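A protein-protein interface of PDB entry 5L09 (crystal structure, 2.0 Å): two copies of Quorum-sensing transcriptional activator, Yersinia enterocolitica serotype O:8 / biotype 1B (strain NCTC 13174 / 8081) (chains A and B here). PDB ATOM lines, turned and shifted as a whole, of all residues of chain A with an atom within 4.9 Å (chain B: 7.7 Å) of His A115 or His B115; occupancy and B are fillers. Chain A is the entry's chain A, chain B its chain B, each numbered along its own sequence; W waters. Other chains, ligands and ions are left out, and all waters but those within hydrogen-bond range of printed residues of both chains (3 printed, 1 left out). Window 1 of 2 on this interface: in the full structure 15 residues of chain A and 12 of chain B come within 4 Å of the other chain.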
ATOM      1  N   LYS A  38       3.245 -18.942  11.284  1.00  0.00           N
ATOM      2  CA  LYS A  38       4.644 -18.640  11.017  1.00  0.00           C
ATOM      3  C   LYS A  38       5.545 -18.856  12.236  1.00  0.00           C
ATOM      4  O   LYS A  38       6.757 -19.013  12.066  1.00  0.00           O
ATOM      5  CB  LYS A  38       4.769 -17.201  10.500  1.00  0.00           C
ATOM      6  CG  LYS A  38       4.123 -17.041   9.086  1.00  0.00           C
ATOM      7  CD  LYS A  38       4.221 -15.612   8.574  1.00  0.00           C
ATOM      8  CE  LYS A  38       3.162 -14.753   9.212  1.00  0.00           C
ATOM      9  NZ  LYS A  38       3.263 -13.344   8.699  1.00  0.00           N
ATOM     10  N   ALA A  73       5.822 -17.127  -0.862  1.00  0.00           N
ATOM     11  CA  ALA A  73       4.669 -16.396  -0.328  1.00  0.00           C
ATOM     12  C   ALA A  73       4.982 -15.770   1.020  1.00  0.00           C
ATOM     13  O   ALA A  73       4.467 -14.687   1.341  1.00  0.00           O
ATOM     14  CB  ALA A  73       3.459 -17.336  -0.180  1.00  0.00           C
ATOM     15  N   LYS A  74       5.846 -16.432   1.796  1.00  0.00           N
ATOM     16  CA  LYS A  74       6.244 -15.976   3.122  1.00  0.00           C
ATOM     17  C   LYS A  74       6.728 -14.531   3.119  1.00  0.00           C
ATOM     18  O   LYS A  74       6.482 -13.793   4.080  1.00  0.00           O
ATOM     19  CB  LYS A  74       7.351 -16.900   3.662  1.00  0.00           C
ATOM     20  CG  LYS A  74       7.919 -16.471   5.001  1.00  0.00           C
ATOM     21  CD  LYS A  74       9.145 -17.296   5.394  1.00  0.00           C
ATOM     22  CE  LYS A  74      10.329 -17.041   4.460  1.00  0.00           C
ATOM     23  NZ  LYS A  74      11.596 -17.630   4.985  1.00  0.00           N
ATOM     24  N   LYS A  76       5.845 -12.192   0.679  1.00  0.00           N
ATOM     25  CA  LYS A  76       5.087 -11.439  -0.317  1.00  0.00           C
ATOM     26  C   LYS A  76       3.760 -11.001   0.282  1.00  0.00           C
ATOM     27  O   LYS A  76       3.297 -11.579   1.264  1.00  0.00           O
ATOM     28  CB  LYS A  76       4.836 -12.284  -1.576  1.00  0.00           C
ATOM     29  CG  LYS A  76       6.120 -12.672  -2.304  1.00  0.00           C
ATOM     30  CD  LYS A  76       6.406 -11.723  -3.441  1.00  0.00           C
ATOM     31  CE  LYS A  76       5.512 -12.043  -4.624  1.00  0.00           C
ATOM     32  NZ  LYS A  76       4.816 -10.844  -5.176  1.00  0.00           N
ATOM     33  N   VAL A  77       3.156  -9.972  -0.320  1.00  0.00           N
ATOM     34  CA  VAL A  77       1.747  -9.655  -0.101  1.00  0.00           C
ATOM     35  C   VAL A  77       0.912  -9.782  -1.367  1.00  0.00           C
ATOM     36  O   VAL A  77      -0.323  -9.902  -1.274  1.00  0.00           O
ATOM     37  CB  VAL A  77       1.574  -8.238   0.500  1.00  0.00           C
ATOM     38  CG1 VAL A  77       2.134  -8.175   1.909  1.00  0.00           C
ATOM     39  CG2 VAL A  77       2.242  -7.141  -0.424  1.00  0.00           C
ATOM     40  N   VAL A 113      -1.679 -14.716  -1.476  1.00  0.00           N
ATOM     41  CA  VAL A 113      -1.161 -14.788  -0.115  1.00  0.00           C
ATOM     42  C   VAL A 113      -1.801 -13.723   0.766  1.00  0.00           C
ATOM     43  O   VAL A 113      -2.174 -12.628   0.320  1.00  0.00           O
ATOM     44  CB  VAL A 113       0.402 -14.683  -0.081  1.00  0.00           C
ATOM     45  CG1 VAL A 113       0.887 -13.342  -0.656  1.00  0.00           C
ATOM     46  CG2 VAL A 113       0.977 -14.933   1.332  1.00  0.00           C
ATOM     47  N   LEU A 114      -1.901 -14.046   2.058  1.00  0.00           N
ATOM     48  CA  LEU A 114      -2.549 -13.190   3.042  1.00  0.00           C
ATOM     49  C   LEU A 114      -1.904 -13.420   4.406  1.00  0.00           C
ATOM     50  O   LEU A 114      -1.989 -14.528   4.942  1.00  0.00           O
ATOM     51  CB  LEU A 114      -4.042 -13.521   3.090  1.00  0.00           C
ATOM     52  CG  LEU A 114      -4.903 -12.752   4.065  1.00  0.00           C
ATOM     53  CD1 LEU A 114      -4.852 -11.296   3.665  1.00  0.00           C
ATOM     54  CD2 LEU A 114      -6.331 -13.292   4.060  1.00  0.00           C
ATOM     55  N   HIS A 115      -1.292 -12.392   4.990  1.00  0.00           N
ATOM     56  CA  HIS A 115      -0.767 -12.480   6.347  1.00  0.00           C
ATOM     57  C   HIS A 115      -1.797 -11.849   7.278  1.00  0.00           C
ATOM     58  O   HIS A 115      -2.353 -10.790   6.964  1.00  0.00           O
ATOM     59  CB  HIS A 115       0.597 -11.798   6.463  1.00  0.00           C
ATOM     60  CG  HIS A 115       1.626 -12.386   5.547  1.00  0.00           C
ATOM     61  ND1 HIS A 115       2.522 -13.349   5.953  1.00  0.00           N
ATOM     62  CD2 HIS A 115       1.852 -12.197   4.226  1.00  0.00           C
ATOM     63  CE1 HIS A 115       3.273 -13.708   4.930  1.00  0.00           C
ATOM     64  NE2 HIS A 115       2.875 -13.037   3.866  1.00  0.00           N
ATOM     65  N   ASP A 116      -2.092 -12.505   8.397  1.00  0.00           N
ATOM     66  CA  ASP A 116      -3.073 -11.928   9.316  1.00  0.00           C
ATOM     67  C   ASP A 116      -2.352 -11.402  10.548  1.00  0.00           C
ATOM     68  O   ASP A 116      -1.120 -11.340  10.590  1.00  0.00           O
ATOM     69  CB  ASP A 116      -4.199 -12.922   9.664  1.00  0.00           C
ATOM     70  CG  ASP A 116      -3.737 -14.137  10.483  1.00  0.00           C
ATOM     71  OD1 ASP A 116      -2.651 -14.124  11.106  1.00  0.00           O
ATOM     72  OD2 ASP A 116      -4.504 -15.132  10.493  1.00  0.00           O
ATOM     73  N   ASN A 117      -3.119 -10.991  11.552  1.00  0.00           N
ATOM     74  CA  ASN A 117      -2.512 -10.428  12.753  1.00  0.00           C
ATOM     75  C   ASN A 117      -2.403 -11.452  13.864  1.00  0.00           C
ATOM     76  O   ASN A 117      -2.250 -11.082  15.030  1.00  0.00           O
ATOM     77  CB  ASN A 117      -3.294  -9.197  13.228  1.00  0.00           C
ATOM     78  CG  ASN A 117      -2.468  -8.307  14.125  1.00  0.00           C
ATOM     79  OD1 ASN A 117      -1.230  -8.364  14.100  1.00  0.00           O
ATOM     80  ND2 ASN A 117      -3.140  -7.485  14.932  1.00  0.00           N
ATOM     81  N   ASN A 120      -0.499 -15.989  11.233  1.00  0.00           N
ATOM     82  CA  ASN A 120      -0.750 -16.971  10.185  1.00  0.00           C
ATOM     83  C   ASN A 120      -0.397 -16.394   8.826  1.00  0.00           C
ATOM     84  O   ASN A 120      -0.541 -15.194   8.585  1.00  0.00           O
ATOM     85  CB  ASN A 120      -2.210 -17.409  10.162  1.00  0.00           C
ATOM     86  CG  ASN A 120      -2.646 -17.987  11.454  1.00  0.00           C
ATOM     87  OD1 ASN A 120      -3.580 -17.485  12.104  1.00  0.00           O
ATOM     88  ND2 ASN A 120      -1.966 -19.039  11.864  1.00  0.00           N
ATOM     89  N   MET A 121       0.053 -17.274   7.935  1.00  0.00           N
ATOM     90  CA  MET A 121       0.095 -16.984   6.527  1.00  0.00           C
ATOM     91  C   MET A 121      -0.920 -17.889   5.854  1.00  0.00           C
ATOM     92  O   MET A 121      -0.857 -19.107   6.005  1.00  0.00           O
ATOM     93  CB  MET A 121       1.488 -17.226   5.956  1.00  0.00           C
ATOM     94  CG  MET A 121       1.539 -16.854   4.487  1.00  0.00           C
ATOM     95  SD  MET A 121       3.165 -17.457   3.634  1.00  0.00           S
ATOM     96  CE  MET A 121       2.845 -19.259   3.541  1.00  0.00           C
ATOM     97  N   MET B  36       2.010   1.217   9.973  1.00  0.00           N
ATOM     98  CA  MET B  36       2.594   1.198  11.299  1.00  0.00           C
ATOM     99  C   MET B  36       3.245  -0.137  11.581  1.00  0.00           C
ATOM    100  O   MET B  36       2.786  -1.205  11.158  1.00  0.00           O
ATOM    101  CB  MET B  36       1.542   1.508  12.364  1.00  0.00           C
ATOM    102  CG  MET B  36       0.202   0.923  12.073  1.00  0.00           C
ATOM    103  SD  MET B  36      -1.173   1.781  13.151  1.00  0.00           S
ATOM    104  CE  MET B  36      -0.627   1.071  14.869  1.00  0.00           C
ATOM    105  N   ILE B  70      -8.465   2.289  13.071  1.00  0.00           N
ATOM    106  CA  ILE B  70      -7.183   1.592  13.156  1.00  0.00           C
ATOM    107  C   ILE B  70      -7.275   0.471  14.182  1.00  0.00           C
ATOM    108  O   ILE B  70      -6.761  -0.630  13.968  1.00  0.00           O
ATOM    109  CB  ILE B  70      -6.052   2.594  13.486  1.00  0.00           C
ATOM    110  CG1 ILE B  70      -5.950   3.683  12.410  1.00  0.00           C
ATOM    111  CG2 ILE B  70      -4.715   1.885  13.675  1.00  0.00           C
ATOM    112  CD1 ILE B  70      -5.732   3.170  10.961  1.00  0.00           C
ATOM    113  N   THR B  72      -9.933  -1.203  14.851  1.00  0.00           N
ATOM    114  CA  THR B  72     -10.697  -2.290  14.234  1.00  0.00           C
ATOM    115  C   THR B  72      -9.843  -3.054  13.227  1.00  0.00           C
ATOM    116  O   THR B  72      -9.869  -4.295  13.188  1.00  0.00           O
ATOM    117  CB  THR B  72     -11.963  -1.722  13.584  1.00  0.00           C
ATOM    118  OG1 THR B  72     -12.770  -1.135  14.605  1.00  0.00           O
ATOM    119  CG2 THR B  72     -12.808  -2.815  12.880  1.00  0.00           C
ATOM    120  N   ALA B  73      -9.078  -2.324  12.411  1.00  0.00           N
ATOM    121  CA  ALA B  73      -8.255  -2.932  11.375  1.00  0.00           C
ATOM    122  C   ALA B  73      -7.277  -3.955  11.951  1.00  0.00           C
ATOM    123  O   ALA B  73      -6.920  -4.918  11.269  1.00  0.00           O
ATOM    124  CB  ALA B  73      -7.499  -1.820  10.631  1.00  0.00           C
ATOM    125  N   LYS B  74      -6.828  -3.758  13.204  1.00  0.00           N
ATOM    126  CA  LYS B  74      -5.944  -4.724  13.850  1.00  0.00           C
ATOM    127  C   LYS B  74      -6.551  -6.118  13.895  1.00  0.00           C
ATOM    128  O   LYS B  74      -5.823  -7.109  13.960  1.00  0.00           O
ATOM    129  CB  LYS B  74      -5.624  -4.285  15.281  1.00  0.00           C
ATOM    130  CG  LYS B  74      -4.666  -3.128  15.368  1.00  0.00           C
ATOM    131  CD  LYS B  74      -4.302  -2.887  16.824  1.00  0.00           C
ATOM    132  CE  LYS B  74      -3.438  -1.649  16.999  1.00  0.00           C
ATOM    133  NZ  LYS B  74      -3.149  -1.416  18.444  1.00  0.00           N
ATOM    134  N   ASP B  75      -7.872  -6.209  13.916  1.00  0.00           N
ATOM    135  CA  ASP B  75      -8.565  -7.476  14.037  1.00  0.00           C
ATOM    136  C   ASP B  75      -9.138  -7.953  12.718  1.00  0.00           C
ATOM    137  O   ASP B  75      -9.889  -8.934  12.706  1.00  0.00           O
ATOM    138  CB  ASP B  75      -9.688  -7.349  15.065  1.00  0.00           C
ATOM    139  CG  ASP B  75      -9.163  -6.983  16.436  1.00  0.00           C
ATOM    140  OD1 ASP B  75      -8.150  -7.594  16.842  1.00  0.00           O
ATOM    141  OD2 ASP B  75      -9.742  -6.076  17.080  1.00  0.00           O
ATOM    142  N   LYS B  76      -8.812  -7.286  11.614  1.00  0.00           N
ATOM    143  CA  LYS B  76      -9.431  -7.584  10.323  1.00  0.00           C
ATOM    144  C   LYS B  76      -8.395  -8.033   9.295  1.00  0.00           C
ATOM    145  O   LYS B  76      -7.221  -7.646   9.356  1.00  0.00           O
ATOM    146  CB  LYS B  76     -10.157  -6.347   9.767  1.00  0.00           C
ATOM    147  CG  LYS B  76     -11.226  -5.752  10.666  1.00  0.00           C
ATOM    148  CD  LYS B  76     -12.438  -6.630  10.681  1.00  0.00           C
ATOM    149  CE  LYS B  76     -13.708  -5.834  10.912  1.00  0.00           C
ATOM    150  NZ  LYS B  76     -14.847  -6.525  10.239  1.00  0.00           N
ATOM    151  N   VAL B  77      -8.855  -8.823   8.324  1.00  0.00           N
ATOM    152  CA  VAL B  77      -8.169  -8.946   7.046  1.00  0.00           C
ATOM    153  C   VAL B  77      -9.004  -8.384   5.906  1.00  0.00           C
ATOM    154  O   VAL B  77      -8.460  -8.178   4.811  1.00  0.00           O
ATOM    155  CB  VAL B  77      -7.793 -10.410   6.731  1.00  0.00           C
ATOM    156  CG1 VAL B  77      -6.725 -10.937   7.718  1.00  0.00           C
ATOM    157  CG2 VAL B  77      -9.050 -11.256   6.747  1.00  0.00           C
ATOM    158  N   ALA B  78     -10.304  -8.205   6.096  1.00  0.00           N
ATOM    159  CA  ALA B  78     -11.205  -7.800   5.033  1.00  0.00           C
ATOM    160  C   ALA B  78     -11.618  -6.350   5.215  1.00  0.00           C
ATOM    161  O   ALA B  78     -11.570  -5.817   6.327  1.00  0.00           O
ATOM    162  CB  ALA B  78     -12.447  -8.691   4.989  1.00  0.00           C
ATOM    163  N   VAL B 113      -7.311  -3.243   4.689  1.00  0.00           N
ATOM    164  CA  VAL B 113      -6.227  -3.582   5.604  1.00  0.00           C
ATOM    165  C   VAL B 113      -5.344  -4.656   4.995  1.00  0.00           C
ATOM    166  O   VAL B 113      -5.790  -5.515   4.228  1.00  0.00           O
ATOM    167  CB  VAL B 113      -6.756  -4.013   7.006  1.00  0.00           C
ATOM    168  CG1 VAL B 113      -7.634  -5.219   6.911  1.00  0.00           C
ATOM    169  CG2 VAL B 113      -5.590  -4.279   8.008  1.00  0.00           C
ATOM    170  N   LEU B 114      -4.063  -4.611   5.375  1.00  0.00           N
ATOM    171  CA  LEU B 114      -3.032  -5.530   4.923  1.00  0.00           C
ATOM    172  C   LEU B 114      -2.009  -5.706   6.042  1.00  0.00           C
ATOM    173  O   LEU B 114      -1.470  -4.716   6.540  1.00  0.00           O
ATOM    174  CB  LEU B 114      -2.356  -4.958   3.665  1.00  0.00           C
ATOM    175  CG  LEU B 114      -1.349  -5.791   2.905  1.00  0.00           C
ATOM    176  CD1 LEU B 114      -2.039  -7.062   2.433  1.00  0.00           C
ATOM    177  CD2 LEU B 114      -0.765  -4.975   1.733  1.00  0.00           C
ATOM    178  N   HIS B 115      -1.713  -6.947   6.416  1.00  0.00           N
ATOM    179  CA  HIS B 115      -0.550  -7.225   7.246  1.00  0.00           C
ATOM    180  C   HIS B 115       0.506  -7.857   6.350  1.00  0.00           C
ATOM    181  O   HIS B 115       0.159  -8.533   5.387  1.00  0.00           O
ATOM    182  CB  HIS B 115      -0.920  -8.132   8.436  1.00  0.00           C
ATOM    183  CG  HIS B 115      -2.038  -7.573   9.281  1.00  0.00           C
ATOM    184  ND1 HIS B 115      -1.815  -6.758  10.372  1.00  0.00           N
ATOM    185  CD2 HIS B 115      -3.383  -7.685   9.167  1.00  0.00           C
ATOM    186  CE1 HIS B 115      -2.970  -6.403  10.901  1.00  0.00           C
ATOM    187  NE2 HIS B 115      -3.940  -6.956  10.193  1.00  0.00           N
ATOM    188  N   ASP B 116       1.795  -7.604   6.627  1.00  0.00           N
ATOM    189  CA  ASP B 116       2.867  -8.260   5.872  1.00  0.00           C
ATOM    190  C   ASP B 116       3.689  -9.133   6.824  1.00  0.00           C
ATOM    191  O   ASP B 116       3.302  -9.369   7.969  1.00  0.00           O
ATOM    192  CB  ASP B 116       3.724  -7.245   5.092  1.00  0.00           C
ATOM    193  CG  ASP B 116       4.486  -6.248   5.990  1.00  0.00           C
ATOM    194  OD1 ASP B 116       4.738  -6.544   7.178  1.00  0.00           O
ATOM    195  OD2 ASP B 116       4.857  -5.159   5.474  1.00  0.00           O
ATOM    196  N   ASN B 117       4.816  -9.655   6.337  1.00  0.00           N
ATOM    197  CA  ASN B 117       5.687 -10.484   7.167  1.00  0.00           C
ATOM    198  C   ASN B 117       6.864  -9.697   7.749  1.00  0.00           C
ATOM    199  O   ASN B 117       7.845 -10.298   8.202  1.00  0.00           O
ATOM    200  CB  ASN B 117       6.206 -11.678   6.369  1.00  0.00           C
ATOM    201  CG  ASN B 117       6.716 -12.809   7.259  1.00  0.00           C
ATOM    202  OD1 ASN B 117       6.185 -13.053   8.342  1.00  0.00           O
ATOM    203  ND2 ASN B 117       7.758 -13.494   6.804  1.00  0.00           N
ATOM    204  N   SER B 118       6.796  -8.368   7.726  1.00  0.00           N
ATOM    205  CA  SER B 118       7.805  -7.504   8.336  1.00  0.00           C
ATOM    206  C   SER B 118       7.274  -6.793   9.570  1.00  0.00           C
ATOM    207  O   SER B 118       7.816  -5.754   9.959  1.00  0.00           O
ATOM    208  CB  SER B 118       8.317  -6.463   7.337  1.00  0.00           C
ATOM    209  OG  SER B 118       8.782  -7.077   6.143  1.00  0.00           O
ATOM    210  N   ASN B 119       6.205  -7.317  10.167  1.00  0.00           N
ATOM    211  CA  ASN B 119       5.500  -6.712  11.298  1.00  0.00           C
ATOM    212  C   ASN B 119       4.812  -5.390  10.960  1.00  0.00           C
ATOM    213  O   ASN B 119       4.574  -4.585  11.861  1.00  0.00           O
ATOM    214  CB  ASN B 119       6.426  -6.487  12.502  1.00  0.00           C
ATOM    215  CG  ASN B 119       7.319  -7.666  12.791  1.00  0.00           C
ATOM    216  OD1 ASN B 119       8.546  -7.532  12.831  1.00  0.00           O
ATOM    217  ND2 ASN B 119       6.712  -8.832  13.006  1.00  0.00           N
ATOM    218  N   ASN B 120       4.492  -5.106   9.701  1.00  0.00           N
ATOM    219  CA  ASN B 120       3.763  -3.879   9.393  1.00  0.00           C
ATOM    220  C   ASN B 120       2.270  -4.165   9.280  1.00  0.00           C
ATOM    221  O   ASN B 120       1.861  -5.216   8.777  1.00  0.00           O
ATOM    222  CB  ASN B 120       4.242  -3.244   8.086  1.00  0.00           C
ATOM    223  CG  ASN B 120       5.730  -2.949   8.082  1.00  0.00           C
ATOM    224  OD1 ASN B 120       6.246  -2.283   8.977  1.00  0.00           O
ATOM    225  ND2 ASN B 120       6.422  -3.442   7.064  1.00  0.00           N
ATOM    226  N   MET B 121       1.459  -3.213   9.728  1.00  0.00           N
ATOM    227  CA  MET B 121       0.074  -3.167   9.298  1.00  0.00           C
ATOM    228  C   MET B 121      -0.106  -1.989   8.356  1.00  0.00           C
ATOM    229  O   MET B 121       0.242  -0.855   8.687  1.00  0.00           O
ATOM    230  CB  MET B 121      -0.897  -3.051  10.481  1.00  0.00           C
ATOM    231  CG  MET B 121      -2.339  -2.894   9.981  1.00  0.00           C
ATOM    232  SD  MET B 121      -3.642  -2.911  11.406  1.00  0.00           S
ATOM    233  CE  MET B 121      -3.299  -1.122  12.079  1.00  0.00           C
ATOM    234  N   ALA B 122      -0.621  -2.237   7.165  1.00  0.00           N
ATOM    235  CA  ALA B 122      -0.890  -1.148   6.238  1.00  0.00           C
ATOM    236  C   ALA B 122      -2.392  -0.983   6.092  1.00  0.00           C
ATOM    237  O   ALA B 122      -3.123  -1.974   5.997  1.00  0.00           O
ATOM    238  CB  ALA B 122      -0.256  -1.404   4.869  1.00  0.00           C
ATOM    239  N   THR B 123      -2.854   0.259   6.085  1.00  0.00           N
ATOM    240  CA  THR B 123      -4.264   0.522   5.822  1.00  0.00           C
ATOM    241  C   THR B 123      -4.399   1.543   4.702  1.00  0.00           C
ATOM    242  O   THR B 123      -3.590   2.468   4.584  1.00  0.00           O
ATOM    243  CB  THR B 123      -5.010   1.023   7.089  1.00  0.00           C
ATOM    244  OG1 THR B 123      -4.384   2.206   7.603  1.00  0.00           O
ATOM    245  CG2 THR B 123      -5.049  -0.069   8.199  1.00  0.00           C
ATOM    246  N   GLN B 148      -8.731  -3.080  -2.879  1.00  0.00           N
ATOM    247  CA  GLN B 148      -7.849  -3.936  -2.077  1.00  0.00           C
ATOM    248  C   GLN B 148      -6.561  -4.245  -2.828  1.00  0.00           C
ATOM    249  O   GLN B 148      -5.461  -4.198  -2.258  1.00  0.00           O
ATOM    250  CB  GLN B 148      -8.571  -5.225  -1.695  1.00  0.00           C
ATOM    251  CG  GLN B 148      -7.716  -6.180  -0.857  1.00  0.00           C
ATOM    252  CD  GLN B 148      -7.469  -5.669   0.564  1.00  0.00           C
ATOM    253  OE1 GLN B 148      -8.237  -4.853   1.093  1.00  0.00           O
ATOM    254  NE2 GLN B 148      -6.403  -6.171   1.196  1.00  0.00           N
ATOM    255  N   LEU B 151      -4.193  -1.314  -2.661  1.00  0.00           N
ATOM    256  CA  LEU B 151      -3.429  -1.315  -1.417  1.00  0.00           C
ATOM    257  C   LEU B 151      -2.307  -2.340  -1.473  1.00  0.00           C
ATOM    258  O   LEU B 151      -1.168  -2.059  -1.071  1.00  0.00           O
ATOM    259  CB  LEU B 151      -4.352  -1.603  -0.226  1.00  0.00           C
ATOM    260  CG  LEU B 151      -3.704  -1.937   1.125  1.00  0.00           C
ATOM    261  CD1 LEU B 151      -2.848  -0.747   1.620  1.00  0.00           C
ATOM    262  CD2 LEU B 151      -4.804  -2.307   2.175  1.00  0.00           C
ATOM    263  N   HIS B 155       1.623  -1.303  -1.468  1.00  0.00           N
ATOM    264  CA  HIS B 155       2.497  -1.727  -0.392  1.00  0.00           C
ATOM    265  C   HIS B 155       3.670  -2.542  -0.925  1.00  0.00           C
ATOM    266  O   HIS B 155       4.797  -2.401  -0.435  1.00  0.00           O
ATOM    267  CB  HIS B 155       1.702  -2.531   0.643  1.00  0.00           C
ATOM    268  CG  HIS B 155       2.457  -2.781   1.903  1.00  0.00           C
ATOM    269  ND1 HIS B 155       2.715  -1.784   2.821  1.00  0.00           N
ATOM    270  CD2 HIS B 155       3.013  -3.911   2.401  1.00  0.00           C
ATOM    271  CE1 HIS B 155       3.412  -2.288   3.825  1.00  0.00           C
ATOM    272  NE2 HIS B 155       3.609  -3.573   3.592  1.00  0.00           N
HETATM  273  O   HOH W   1      -3.885  -8.904   5.797  1.00  0.00           O
HETATM  274  O   HOH W   2      -1.149  -9.930   3.637  1.00  0.00           O
HETATM  275  O   HOH W   3       5.119 -10.228   3.553  1.00  0.00           O
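Lys A74 touches Asn B117, and with the chains exchanged Asn A117 touches Lys B74.
Val A77 touches Asp B116, and with the chains exchanged Asp A116 touches Val B77.
His A115 touches Asp B116, and with the chains exchanged Asp A116 touches His B115.
His A115 touches Asn B117, and with the chains exchanged Asn A117 touches His B115.
Positions printed for both chains: 73, 74, 76, 77, 113, 114, 115, 116, 117, 120 and 121.
Of the 10 pairs that touch across the chains among the printed residues, 9 have their exchanged pair printed and touching as well.
The side-chain amide oxygen (OD1) of Asn B117 sits at hydrogen-bond distance from the side-chain amino group (NZ) of Lys A38 (3.0 Å).
The side-chain amide nitrogen (ND2) of Asn B117 lies within hydrogen-bond range of the backbone carbonyl oxygen (O) of Lys A74.
O of Lys B74 is in hydrogen-bond range of ND2 of Asn A117 (2.9 Å).
Water W2 lies within hydrogen-bond range of the backbone carbonyl oxygen (O) of His B115 (2.6 Å) and the backbone NH (N) of His A115 (2.8 Å).
Water W1 bridges the backbone carbonyl oxygen (O) of His A115 (2.7 Å) and the backbone NH (N) of His B115 (3.0 Å).
Water W3 lies within hydrogen-bond range of N of Asn B117 (2.9 Å) and O of Lys A76 (3.2 Å).
NZ of Lys A38 sits at hydrogen-bond distance from ND1 of His A115 (2.8 Å).
N of Lys A74 is in hydrogen-bond range of SD of Met A121 (3.4 Å).
O of Lys A76 lies within hydrogen-bond range of NE2 of His A115, at 3.0 Å.
The side-chain carboxylate of Asp B116 is in hydrogen-bond range of the backbone NH of Ser B118 (2.8 Å).
N of Asn B119 is in hydrogen-bond range of OD1 of Asp B116 (3.4 Å).
OD2 of Asp B116 lies within hydrogen-bond range of NE2 of His B155 (2.8 Å).
Among the printed residues, pairs that only touch across the chains: Val A77 with Asp B116, His A115 with His B115, His A115 with Asp B116, His A115 with Asn B117, Asp A116 with Val B77, Asp A116 with His B115 and Asn A117 with His B115.
Of the 23 printed residues of chain B, 5 touch a printed residue of chain A.
Hydrophobic or aromatic side chains of chain B within 4 Å of the printed part of chain A: Val B77 and His B115.
Along chain B the printed residues that touch a printed residue of chain A span positions 74 to 117.
Hydrophobic or aromatic side chains of chain A that line the printed part of chain B: Val A77 and His A115.
Among the printed residues, 10 pairs touch across the chains.
Printed residues of chain B within 4 Å of Lys A74: Asn B117.
Of the printed residues of chain B, Asp A116 touches Val B77 and His B115.
Of the printed residues of chain A, Lys B74 touches Asn A117 (2.9 Å).
Of the printed residues of chain A, Asp B116 touches Val A77 (3.7 Å) and His A115 (3.9 Å).
Of the printed residues of chain A, Asn B117 touches Lys A38 (3.0 Å), Lys A74 (3.0 Å) and His A115 (3.8 Å).
The nearest printed residue of chain A that does not touch His B115 is Val A77 (4.02 Å).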
